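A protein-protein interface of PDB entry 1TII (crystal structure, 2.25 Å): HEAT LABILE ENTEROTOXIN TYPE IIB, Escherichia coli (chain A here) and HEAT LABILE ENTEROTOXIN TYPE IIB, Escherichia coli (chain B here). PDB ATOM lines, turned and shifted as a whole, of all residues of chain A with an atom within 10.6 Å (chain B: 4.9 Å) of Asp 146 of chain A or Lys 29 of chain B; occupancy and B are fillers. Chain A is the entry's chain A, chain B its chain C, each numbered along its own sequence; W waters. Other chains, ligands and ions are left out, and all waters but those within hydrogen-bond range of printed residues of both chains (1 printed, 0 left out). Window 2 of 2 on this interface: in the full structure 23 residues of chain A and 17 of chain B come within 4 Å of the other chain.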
ATOM      1  N   GLU A  30      13.832  11.192 -10.849  1.00  0.00           N
ATOM      2  CA  GLU A  30      15.155  10.625 -10.977  1.00  0.00           C
ATOM      3  C   GLU A  30      15.509   9.499 -10.007  1.00  0.00           C
ATOM      4  O   GLU A  30      16.441   8.742 -10.265  1.00  0.00           O
ATOM      5  CB  GLU A  30      16.205  11.733 -10.901  1.00  0.00           C
ATOM      6  CG  GLU A  30      16.421  12.507 -12.208  1.00  0.00           C
ATOM      7  CD  GLU A  30      17.000  11.652 -13.356  1.00  0.00           C
ATOM      8  OE1 GLU A  30      17.761  10.686 -13.078  1.00  0.00           O
ATOM      9  OE2 GLU A  30      16.704  11.963 -14.543  1.00  0.00           O
ATOM     10  N   ALA A  87       7.489  20.267 -23.191  1.00  0.00           N
ATOM     11  CA  ALA A  87       8.274  20.313 -24.434  1.00  0.00           C
ATOM     12  C   ALA A  87       8.419  18.911 -25.009  1.00  0.00           C
ATOM     13  O   ALA A  87       8.474  17.928 -24.262  1.00  0.00           O
ATOM     14  CB  ALA A  87       9.633  20.896 -24.187  1.00  0.00           C
ATOM     15  N   ALA A  88       8.524  18.831 -26.327  1.00  0.00           N
ATOM     16  CA  ALA A  88       8.658  17.553 -27.014  1.00  0.00           C
ATOM     17  C   ALA A  88      10.016  16.916 -26.739  1.00  0.00           C
ATOM     18  O   ALA A  88      11.032  17.604 -26.617  1.00  0.00           O
ATOM     19  CB  ALA A  88       8.441  17.738 -28.498  1.00  0.00           C
ATOM     20  N   ALA A  89      10.009  15.602 -26.557  1.00  0.00           N
ATOM     21  CA  ALA A  89      11.231  14.838 -26.314  1.00  0.00           C
ATOM     22  C   ALA A  89      10.880  13.365 -26.597  1.00  0.00           C
ATOM     23  O   ALA A  89       9.688  13.005 -26.642  1.00  0.00           O
ATOM     24  CB  ALA A  89      11.726  15.024 -24.888  1.00  0.00           C
ATOM     25  N   PRO A  90      11.901  12.503 -26.789  1.00  0.00           N
ATOM     26  CA  PRO A  90      11.689  11.081 -27.078  1.00  0.00           C
ATOM     27  C   PRO A  90      11.103  10.218 -25.982  1.00  0.00           C
ATOM     28  O   PRO A  90      11.135   9.002 -26.108  1.00  0.00           O
ATOM     29  CB  PRO A  90      13.079  10.602 -27.477  1.00  0.00           C
ATOM     30  CG  PRO A  90      13.748  11.838 -27.979  1.00  0.00           C
ATOM     31  CD  PRO A  90      13.319  12.845 -26.964  1.00  0.00           C
ATOM     32  N   SER A 120      12.356  19.711 -15.504  1.00  0.00           N
ATOM     33  CA  SER A 120      13.053  20.508 -16.517  1.00  0.00           C
ATOM     34  C   SER A 120      12.405  20.478 -17.883  1.00  0.00           C
ATOM     35  O   SER A 120      12.770  21.265 -18.753  1.00  0.00           O
ATOM     36  CB  SER A 120      14.492  20.025 -16.660  1.00  0.00           C
ATOM     37  OG  SER A 120      14.543  18.636 -16.996  1.00  0.00           O
ATOM     38  N   GLN A 121      11.472  19.545 -18.092  1.00  0.00           N
ATOM     39  CA  GLN A 121      10.773  19.417 -19.371  1.00  0.00           C
ATOM     40  C   GLN A 121       9.473  20.210 -19.346  1.00  0.00           C
ATOM     41  O   GLN A 121       8.888  20.477 -20.396  1.00  0.00           O
ATOM     42  CB  GLN A 121      10.493  17.937 -19.687  1.00  0.00           C
ATOM     43  CG  GLN A 121       9.994  17.618 -21.123  1.00  0.00           C
ATOM     44  CD  GLN A 121       9.803  16.118 -21.384  1.00  0.00           C
ATOM     45  OE1 GLN A 121      10.176  15.268 -20.566  1.00  0.00           O
ATOM     46  NE2 GLN A 121       9.223  15.795 -22.526  1.00  0.00           N
ATOM     47  N   ILE A 123       7.509  23.326 -19.366  1.00  0.00           N
ATOM     48  CA  ILE A 123       7.674  24.722 -19.746  1.00  0.00           C
ATOM     49  C   ILE A 123       6.920  25.697 -18.842  1.00  0.00           C
ATOM     50  O   ILE A 123       7.409  26.770 -18.536  1.00  0.00           O
ATOM     51  CB  ILE A 123       7.194  24.946 -21.159  1.00  0.00           C
ATOM     52  CG1 ILE A 123       7.994  24.071 -22.114  1.00  0.00           C
ATOM     53  CG2 ILE A 123       7.324  26.395 -21.528  1.00  0.00           C
ATOM     54  CD1 ILE A 123       7.489  24.137 -23.530  1.00  0.00           C
ATOM     55  N   ASN A 140       7.712  28.070 -15.924  1.00  0.00           N
ATOM     56  CA  ASN A 140       8.408  27.234 -14.963  1.00  0.00           C
ATOM     57  C   ASN A 140       9.864  27.645 -14.973  1.00  0.00           C
ATOM     58  O   ASN A 140      10.555  27.542 -15.990  1.00  0.00           O
ATOM     59  CB  ASN A 140       8.267  25.758 -15.318  1.00  0.00           C
ATOM     60  CG  ASN A 140       9.164  24.861 -14.483  1.00  0.00           C
ATOM     61  OD1 ASN A 140       9.578  25.219 -13.377  1.00  0.00           O
ATOM     62  ND2 ASN A 140       9.484  23.689 -15.017  1.00  0.00           N
ATOM     63  N   ARG A 141      10.336  28.116 -13.829  1.00  0.00           N
ATOM     64  CA  ARG A 141      11.714  28.573 -13.715  1.00  0.00           C
ATOM     65  C   ARG A 141      12.749  27.473 -13.847  1.00  0.00           C
ATOM     66  O   ARG A 141      13.883  27.755 -14.178  1.00  0.00           O
ATOM     67  CB  ARG A 141      11.906  29.372 -12.425  1.00  0.00           C
ATOM     68  CG  ARG A 141      11.243  30.755 -12.475  1.00  0.00           C
ATOM     69  CD  ARG A 141      11.070  31.317 -11.070  1.00  0.00           C
ATOM     70  NE  ARG A 141      10.714  32.741 -11.056  1.00  0.00           N
ATOM     71  CZ  ARG A 141      10.846  33.546  -9.990  1.00  0.00           C
ATOM     72  NH1 ARG A 141      11.336  33.078  -8.828  1.00  0.00           N
ATOM     73  NH2 ARG A 141      10.476  34.829 -10.077  1.00  0.00           N
ATOM     74  N   ASP A 142      12.348  26.225 -13.622  1.00  0.00           N
ATOM     75  CA  ASP A 142      13.260  25.090 -13.744  1.00  0.00           C
ATOM     76  C   ASP A 142      13.258  24.457 -15.141  1.00  0.00           C
ATOM     77  O   ASP A 142      13.865  23.425 -15.353  1.00  0.00           O
ATOM     78  CB  ASP A 142      12.944  24.049 -12.684  1.00  0.00           C
ATOM     79  CG  ASP A 142      13.152  24.573 -11.287  1.00  0.00           C
ATOM     80  OD1 ASP A 142      14.285  24.997 -10.978  1.00  0.00           O
ATOM     81  OD2 ASP A 142      12.186  24.572 -10.494  1.00  0.00           O
ATOM     82  N   TYR A 143      12.548  25.069 -16.084  1.00  0.00           N
ATOM     83  CA  TYR A 143      12.517  24.578 -17.443  1.00  0.00           C
ATOM     84  C   TYR A 143      13.919  24.802 -17.991  1.00  0.00           C
ATOM     85  O   TYR A 143      14.493  25.856 -17.765  1.00  0.00           O
ATOM     86  CB  TYR A 143      11.530  25.377 -18.283  1.00  0.00           C
ATOM     87  CG  TYR A 143      11.546  24.972 -19.737  1.00  0.00           C
ATOM     88  CD1 TYR A 143      11.423  23.637 -20.106  1.00  0.00           C
ATOM     89  CD2 TYR A 143      11.730  25.911 -20.738  1.00  0.00           C
ATOM     90  CE1 TYR A 143      11.483  23.252 -21.426  1.00  0.00           C
ATOM     91  CE2 TYR A 143      11.792  25.535 -22.058  1.00  0.00           C
ATOM     92  CZ  TYR A 143      11.669  24.199 -22.391  1.00  0.00           C
ATOM     93  OH  TYR A 143      11.740  23.820 -23.704  1.00  0.00           O
ATOM     94  N   ARG A 144      14.488  23.792 -18.649  1.00  0.00           N
ATOM     95  CA  ARG A 144      15.826  23.890 -19.231  1.00  0.00           C
ATOM     96  C   ARG A 144      15.728  23.846 -20.755  1.00  0.00           C
ATOM     97  O   ARG A 144      15.768  22.781 -21.353  1.00  0.00           O
ATOM     98  CB  ARG A 144      16.717  22.753 -18.735  1.00  0.00           C
ATOM     99  CG  ARG A 144      16.964  22.700 -17.234  1.00  0.00           C
ATOM    100  CD  ARG A 144      17.986  23.732 -16.736  1.00  0.00           C
ATOM    101  NE  ARG A 144      17.354  25.030 -16.507  1.00  0.00           N
ATOM    102  CZ  ARG A 144      17.125  25.586 -15.314  1.00  0.00           C
ATOM    103  NH1 ARG A 144      17.493  24.989 -14.177  1.00  0.00           N
ATOM    104  NH2 ARG A 144      16.409  26.705 -15.273  1.00  0.00           N
ATOM    105  N   ARG A 145      15.607  25.009 -21.377  1.00  0.00           N
ATOM    106  CA  ARG A 145      15.484  25.113 -22.812  1.00  0.00           C
ATOM    107  C   ARG A 145      16.660  24.524 -23.570  1.00  0.00           C
ATOM    108  O   ARG A 145      16.486  23.946 -24.642  1.00  0.00           O
ATOM    109  CB  ARG A 145      15.287  26.569 -23.226  1.00  0.00           C
ATOM    110  CG  ARG A 145      16.457  27.472 -22.931  1.00  0.00           C
ATOM    111  CD  ARG A 145      16.114  28.862 -23.377  1.00  0.00           C
ATOM    112  NE  ARG A 145      17.067  29.888 -22.944  1.00  0.00           N
ATOM    113  CZ  ARG A 145      16.701  31.061 -22.427  1.00  0.00           C
ATOM    114  NH1 ARG A 145      15.418  31.314 -22.215  1.00  0.00           N
ATOM    115  NH2 ARG A 145      17.607  31.961 -22.073  1.00  0.00           N
ATOM    116  N   ASP A 146      17.860  24.677 -23.035  1.00  0.00           N
ATOM    117  CA  ASP A 146      19.037  24.144 -23.707  1.00  0.00           C
ATOM    118  C   ASP A 146      19.008  22.614 -23.829  1.00  0.00           C
ATOM    119  O   ASP A 146      19.707  22.048 -24.652  1.00  0.00           O
ATOM    120  CB  ASP A 146      20.316  24.602 -22.992  1.00  0.00           C
ATOM    121  CG  ASP A 146      20.360  24.182 -21.536  1.00  0.00           C
ATOM    122  OD1 ASP A 146      19.297  24.096 -20.892  1.00  0.00           O
ATOM    123  OD2 ASP A 146      21.473  23.953 -21.024  1.00  0.00           O
ATOM    124  N   LEU A 147      18.233  21.954 -22.983  1.00  0.00           N
ATOM    125  CA  LEU A 147      18.141  20.504 -23.021  1.00  0.00           C
ATOM    126  C   LEU A 147      17.046  19.977 -23.957  1.00  0.00           C
ATOM    127  O   LEU A 147      17.101  18.820 -24.409  1.00  0.00           O
ATOM    128  CB  LEU A 147      17.869  19.937 -21.622  1.00  0.00           C
ATOM    129  CG  LEU A 147      18.814  20.123 -20.441  1.00  0.00           C
ATOM    130  CD1 LEU A 147      18.376  19.166 -19.351  1.00  0.00           C
ATOM    131  CD2 LEU A 147      20.261  19.842 -20.847  1.00  0.00           C
ATOM    132  N   PHE A 148      16.038  20.804 -24.213  1.00  0.00           N
ATOM    133  CA  PHE A 148      14.925  20.372 -25.022  1.00  0.00           C
ATOM    134  C   PHE A 148      14.722  21.028 -26.372  1.00  0.00           C
ATOM    135  O   PHE A 148      13.907  20.564 -27.148  1.00  0.00           O
ATOM    136  CB  PHE A 148      13.660  20.408 -24.178  1.00  0.00           C
ATOM    137  CG  PHE A 148      13.681  19.415 -23.068  1.00  0.00           C
ATOM    138  CD1 PHE A 148      13.405  18.079 -23.317  1.00  0.00           C
ATOM    139  CD2 PHE A 148      14.115  19.776 -21.808  1.00  0.00           C
ATOM    140  CE1 PHE A 148      13.578  17.120 -22.333  1.00  0.00           C
ATOM    141  CE2 PHE A 148      14.291  18.816 -20.812  1.00  0.00           C
ATOM    142  CZ  PHE A 148      14.026  17.484 -21.079  1.00  0.00           C
ATOM    143  N   ARG A 149      15.488  22.063 -26.679  1.00  0.00           N
ATOM    144  CA  ARG A 149      15.367  22.757 -27.950  1.00  0.00           C
ATOM    145  C   ARG A 149      15.547  21.795 -29.133  1.00  0.00           C
ATOM    146  O   ARG A 149      16.541  21.091 -29.248  1.00  0.00           O
ATOM    147  CB  ARG A 149      16.411  23.880 -28.010  1.00  0.00           C
ATOM    148  CG  ARG A 149      16.570  24.609 -29.352  1.00  0.00           C
ATOM    149  CD  ARG A 149      15.332  25.406 -29.742  1.00  0.00           C
ATOM    150  NE  ARG A 149      14.752  26.101 -28.595  1.00  0.00           N
ATOM    151  CZ  ARG A 149      15.042  27.350 -28.244  1.00  0.00           C
ATOM    152  NH1 ARG A 149      15.905  28.064 -28.958  1.00  0.00           N
ATOM    153  NH2 ARG A 149      14.499  27.865 -27.148  1.00  0.00           N
ATOM    154  N   GLY A 150      14.534  21.720 -29.980  1.00  0.00           N
ATOM    155  CA  GLY A 150      14.626  20.875 -31.158  1.00  0.00           C
ATOM    156  C   GLY A 150      14.520  19.358 -31.041  1.00  0.00           C
ATOM    157  O   GLY A 150      14.966  18.648 -31.940  1.00  0.00           O
ATOM    158  N   LEU A 151      14.001  18.856 -29.927  1.00  0.00           N
ATOM    159  CA  LEU A 151      13.821  17.429 -29.762  1.00  0.00           C
ATOM    160  C   LEU A 151      12.406  17.166 -30.263  1.00  0.00           C
ATOM    161  O   LEU A 151      11.671  18.109 -30.565  1.00  0.00           O
ATOM    162  CB  LEU A 151      13.979  17.024 -28.295  1.00  0.00           C
ATOM    163  CG  LEU A 151      15.371  17.156 -27.675  1.00  0.00           C
ATOM    164  CD1 LEU A 151      15.472  16.384 -26.376  1.00  0.00           C
ATOM    165  CD2 LEU A 151      16.372  16.612 -28.637  1.00  0.00           C
ATOM    166  N   SER A 152      12.059  15.908 -30.494  1.00  0.00           N
ATOM    167  CA  SER A 152      10.708  15.608 -30.922  1.00  0.00           C
ATOM    168  C   SER A 152      10.328  14.308 -30.290  1.00  0.00           C
ATOM    169  O   SER A 152      11.139  13.682 -29.621  1.00  0.00           O
ATOM    170  CB  SER A 152      10.589  15.535 -32.441  1.00  0.00           C
ATOM    171  OG  SER A 152      11.472  14.577 -32.973  1.00  0.00           O
ATOM    172  N   LYS B  24      19.358   8.721 -18.442  1.00  0.00           N
ATOM    173  CA  LYS B  24      20.808   8.897 -18.601  1.00  0.00           C
ATOM    174  C   LYS B  24      21.086   9.951 -19.650  1.00  0.00           C
ATOM    175  O   LYS B  24      22.013  10.731 -19.523  1.00  0.00           O
ATOM    176  CB  LYS B  24      21.513   7.617 -19.048  1.00  0.00           C
ATOM    177  CG  LYS B  24      21.522   6.476 -18.069  1.00  0.00           C
ATOM    178  CD  LYS B  24      22.582   5.467 -18.503  1.00  0.00           C
ATOM    179  CE  LYS B  24      22.350   4.079 -17.912  1.00  0.00           C
ATOM    180  NZ  LYS B  24      21.410   3.225 -18.725  1.00  0.00           N
ATOM    181  N   TYR B  25      20.311   9.931 -20.721  1.00  0.00           N
ATOM    182  CA  TYR B  25      20.462  10.893 -21.802  1.00  0.00           C
ATOM    183  C   TYR B  25      20.344  12.346 -21.296  1.00  0.00           C
ATOM    184  O   TYR B  25      21.112  13.229 -21.672  1.00  0.00           O
ATOM    185  CB  TYR B  25      19.385  10.634 -22.851  1.00  0.00           C
ATOM    186  CG  TYR B  25      19.359  11.670 -23.942  1.00  0.00           C
ATOM    187  CD1 TYR B  25      20.432  11.798 -24.818  1.00  0.00           C
ATOM    188  CD2 TYR B  25      18.278  12.545 -24.082  1.00  0.00           C
ATOM    189  CE1 TYR B  25      20.444  12.770 -25.815  1.00  0.00           C
ATOM    190  CE2 TYR B  25      18.276  13.523 -25.078  1.00  0.00           C
ATOM    191  CZ  TYR B  25      19.369  13.623 -25.942  1.00  0.00           C
ATOM    192  OH  TYR B  25      19.393  14.560 -26.949  1.00  0.00           O
ATOM    193  N   ILE B  26      19.319  12.598 -20.495  1.00  0.00           N
ATOM    194  CA  ILE B  26      19.101  13.920 -19.929  1.00  0.00           C
ATOM    195  C   ILE B  26      20.290  14.319 -19.008  1.00  0.00           C
ATOM    196  O   ILE B  26      20.839  15.421 -19.144  1.00  0.00           O
ATOM    197  CB  ILE B  26      17.723  13.971 -19.183  1.00  0.00           C
ATOM    198  CG1 ILE B  26      16.574  13.989 -20.185  1.00  0.00           C
ATOM    199  CG2 ILE B  26      17.613  15.197 -18.326  1.00  0.00           C
ATOM    200  CD1 ILE B  26      16.708  15.052 -21.247  1.00  0.00           C
ATOM    201  N   LYS B  27      20.728  13.402 -18.140  1.00  0.00           N
ATOM    202  CA  LYS B  27      21.839  13.659 -17.218  1.00  0.00           C
ATOM    203  C   LYS B  27      23.122  13.985 -17.911  1.00  0.00           C
ATOM    204  O   LYS B  27      23.905  14.806 -17.437  1.00  0.00           O
ATOM    205  CB  LYS B  27      22.117  12.467 -16.307  1.00  0.00           C
ATOM    206  CG  LYS B  27      21.245  12.393 -15.093  1.00  0.00           C
ATOM    207  CD  LYS B  27      22.057  12.444 -13.796  1.00  0.00           C
ATOM    208  CE  LYS B  27      22.429  11.042 -13.299  1.00  0.00           C
ATOM    209  NZ  LYS B  27      23.058  11.011 -11.930  1.00  0.00           N
ATOM    210  N   ARG B  28      23.376  13.297 -19.009  1.00  0.00           N
ATOM    211  CA  ARG B  28      24.602  13.519 -19.738  1.00  0.00           C
ATOM    212  C   ARG B  28      24.533  14.785 -20.544  1.00  0.00           C
ATOM    213  O   ARG B  28      25.543  15.459 -20.692  1.00  0.00           O
ATOM    214  CB  ARG B  28      24.940  12.303 -20.605  1.00  0.00           C
ATOM    215  CG  ARG B  28      25.202  11.085 -19.765  1.00  0.00           C
ATOM    216  CD  ARG B  28      25.549   9.879 -20.563  1.00  0.00           C
ATOM    217  NE  ARG B  28      25.634   8.736 -19.662  1.00  0.00           N
ATOM    218  CZ  ARG B  28      26.016   7.509 -20.020  1.00  0.00           C
ATOM    219  NH1 ARG B  28      26.358   7.252 -21.286  1.00  0.00           N
ATOM    220  NH2 ARG B  28      26.070   6.542 -19.102  1.00  0.00           N
ATOM    221  N   LYS B  29      23.357  15.119 -21.061  1.00  0.00           N
ATOM    222  CA  LYS B  29      23.211  16.361 -21.813  1.00  0.00           C
ATOM    223  C   LYS B  29      23.347  17.562 -20.843  1.00  0.00           C
ATOM    224  O   LYS B  29      24.019  18.557 -21.139  1.00  0.00           O
ATOM    225  CB  LYS B  29      21.869  16.416 -22.532  1.00  0.00           C
ATOM    226  CG  LYS B  29      21.914  17.385 -23.688  1.00  0.00           C
ATOM    227  CD  LYS B  29      20.579  17.517 -24.332  1.00  0.00           C
ATOM    228  CE  LYS B  29      20.632  18.436 -25.517  1.00  0.00           C
ATOM    229  NZ  LYS B  29      19.287  18.435 -26.168  1.00  0.00           N
ATOM    230  N   PHE B  30      22.699  17.468 -19.688  1.00  0.00           N
ATOM    231  CA  PHE B  30      22.806  18.511 -18.681  1.00  0.00           C
ATOM    232  C   PHE B  30      24.282  18.669 -18.296  1.00  0.00           C
ATOM    233  O   PHE B  30      24.820  19.768 -18.342  1.00  0.00           O
ATOM    234  CB  PHE B  30      22.004  18.144 -17.447  1.00  0.00           C
ATOM    235  CG  PHE B  30      22.329  18.998 -16.266  1.00  0.00           C
ATOM    236  CD1 PHE B  30      21.777  20.267 -16.142  1.00  0.00           C
ATOM    237  CD2 PHE B  30      23.247  18.563 -15.311  1.00  0.00           C
ATOM    238  CE1 PHE B  30      22.132  21.093 -15.098  1.00  0.00           C
ATOM    239  CE2 PHE B  30      23.609  19.380 -14.268  1.00  0.00           C
ATOM    240  CZ  PHE B  30      23.047  20.656 -14.163  1.00  0.00           C
ATOM    241  N   THR B  31      24.929  17.559 -17.936  1.00  0.00           N
ATOM    242  CA  THR B  31      26.346  17.550 -17.580  1.00  0.00           C
ATOM    243  C   THR B  31      27.192  18.261 -18.635  1.00  0.00           C
ATOM    244  O   THR B  31      28.057  19.072 -18.301  1.00  0.00           O
ATOM    245  CB  THR B  31      26.878  16.111 -17.439  1.00  0.00           C
ATOM    246  OG1 THR B  31      26.268  15.484 -16.314  1.00  0.00           O
ATOM    247  CG2 THR B  31      28.376  16.097 -17.233  1.00  0.00           C
ATOM    248  N   LEU B  32      26.939  17.954 -19.901  1.00  0.00           N
ATOM    249  CA  LEU B  32      27.678  18.537 -21.012  1.00  0.00           C
ATOM    250  C   LEU B  32      27.504  20.046 -21.113  1.00  0.00           C
ATOM    251  O   LEU B  32      28.454  20.758 -21.404  1.00  0.00           O
ATOM    252  CB  LEU B  32      27.249  17.871 -22.329  1.00  0.00           C
ATOM    253  CG  LEU B  32      27.749  18.438 -23.662  1.00  0.00           C
ATOM    254  CD1 LEU B  32      29.250  18.249 -23.768  1.00  0.00           C
ATOM    255  CD2 LEU B  32      27.037  17.755 -24.826  1.00  0.00           C
ATOM    256  N   MET B  33      26.278  20.529 -20.959  1.00  0.00           N
ATOM    257  CA  MET B  33      26.046  21.966 -21.033  1.00  0.00           C
ATOM    258  C   MET B  33      26.702  22.649 -19.827  1.00  0.00           C
ATOM    259  O   MET B  33      27.253  23.728 -19.965  1.00  0.00           O
ATOM    260  CB  MET B  33      24.548  22.283 -21.095  1.00  0.00           C
ATOM    261  CG  MET B  33      23.816  21.656 -22.276  1.00  0.00           C
ATOM    262  SD  MET B  33      24.246  22.341 -23.897  1.00  0.00           S
ATOM    263  CE  MET B  33      25.263  21.099 -24.487  1.00  0.00           C
HETATM  264  O   HOH W   1      18.820  20.780 -27.481  1.00  0.00           O
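O of Leu 147 of chain A sits at hydrogen-bond distance from NZ of Lys 29 of chain B (2.8 Å).
Water W1 lies within hydrogen-bond range of the side-chain amino group of Lys 29 of chain B, the backbone carbonyl oxygen of Arg 149 of chain A and the backbone carbonyl oxygen of Asp 146 of chain A.
Of chain B, only Lys 29 (3.8 Å) and Met 33 (3.5 Å) come within 4 Å of Asp 146 of chain A.
Of the printed residues of chain B, Leu 147 of chain A touches Lys 29 (2.8 Å) and Phe 30 (3.6 Å).
Of the printed residues of chain B, Phe 148 of chain A touches Ile 26.
No residue of chain A comes within 4 Å of Tyr 25 of chain B.
Ile 26 of chain B touches just one residue of chain A: Phe 148.
Printed residues of chain A within 4 Å of Phe 30 of chain B: Leu 147 (3.6 Å).
No residue of chain A comes within 4 Å of Leu 32 of chain B.
Met 33 of chain B touches just one residue of chain A: Asp 146.
The nearest printed residue of chain B that does not touch Asp 146 of chain A is Phe 30 of chain B (6.0 Å).
The nearest residue of chain A that does not touch Lys 29 of chain B is Leu 151 of chain A (4.2 Å).
The nearest printed residue of chain B that does not touch Phe 148 of chain A is Lys 29 of chain B (4.5 Å).
Of the 10 printed residues of chain B, 4 touch a printed residue of chain A.
Printed residues of chain B that touch a printed residue of chain A: Ile 26, Lys 29, Phe 30 and Met 33.
Hydrophobic or aromatic side chains of chain B that line the printed part of chain A: Ile 26 and Met 33.
Of the 21 printed residues of chain A, 3 touch a printed residue of chain B.
Hydrophobic or aromatic side chains of chain A that line the printed part of chain B: Leu 147 and Phe 148.
Among the printed residues, no Asp or Glu carboxylate lies within 4 Å of a Lys or Arg side-chain nitrogen of the other chain.
Among the printed residues, merely in contact across the chains: Asp 146 of chain A with Lys 29 of chain B (3.8 Å), Asp 146 of chain A with Met 33 of chain B (3.5 Å), Leu 147 of chain A with Phe 30 of chain B (3.6 Å) and Phe 148 of chain A with Ile 26 of chain B (3.6 Å).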
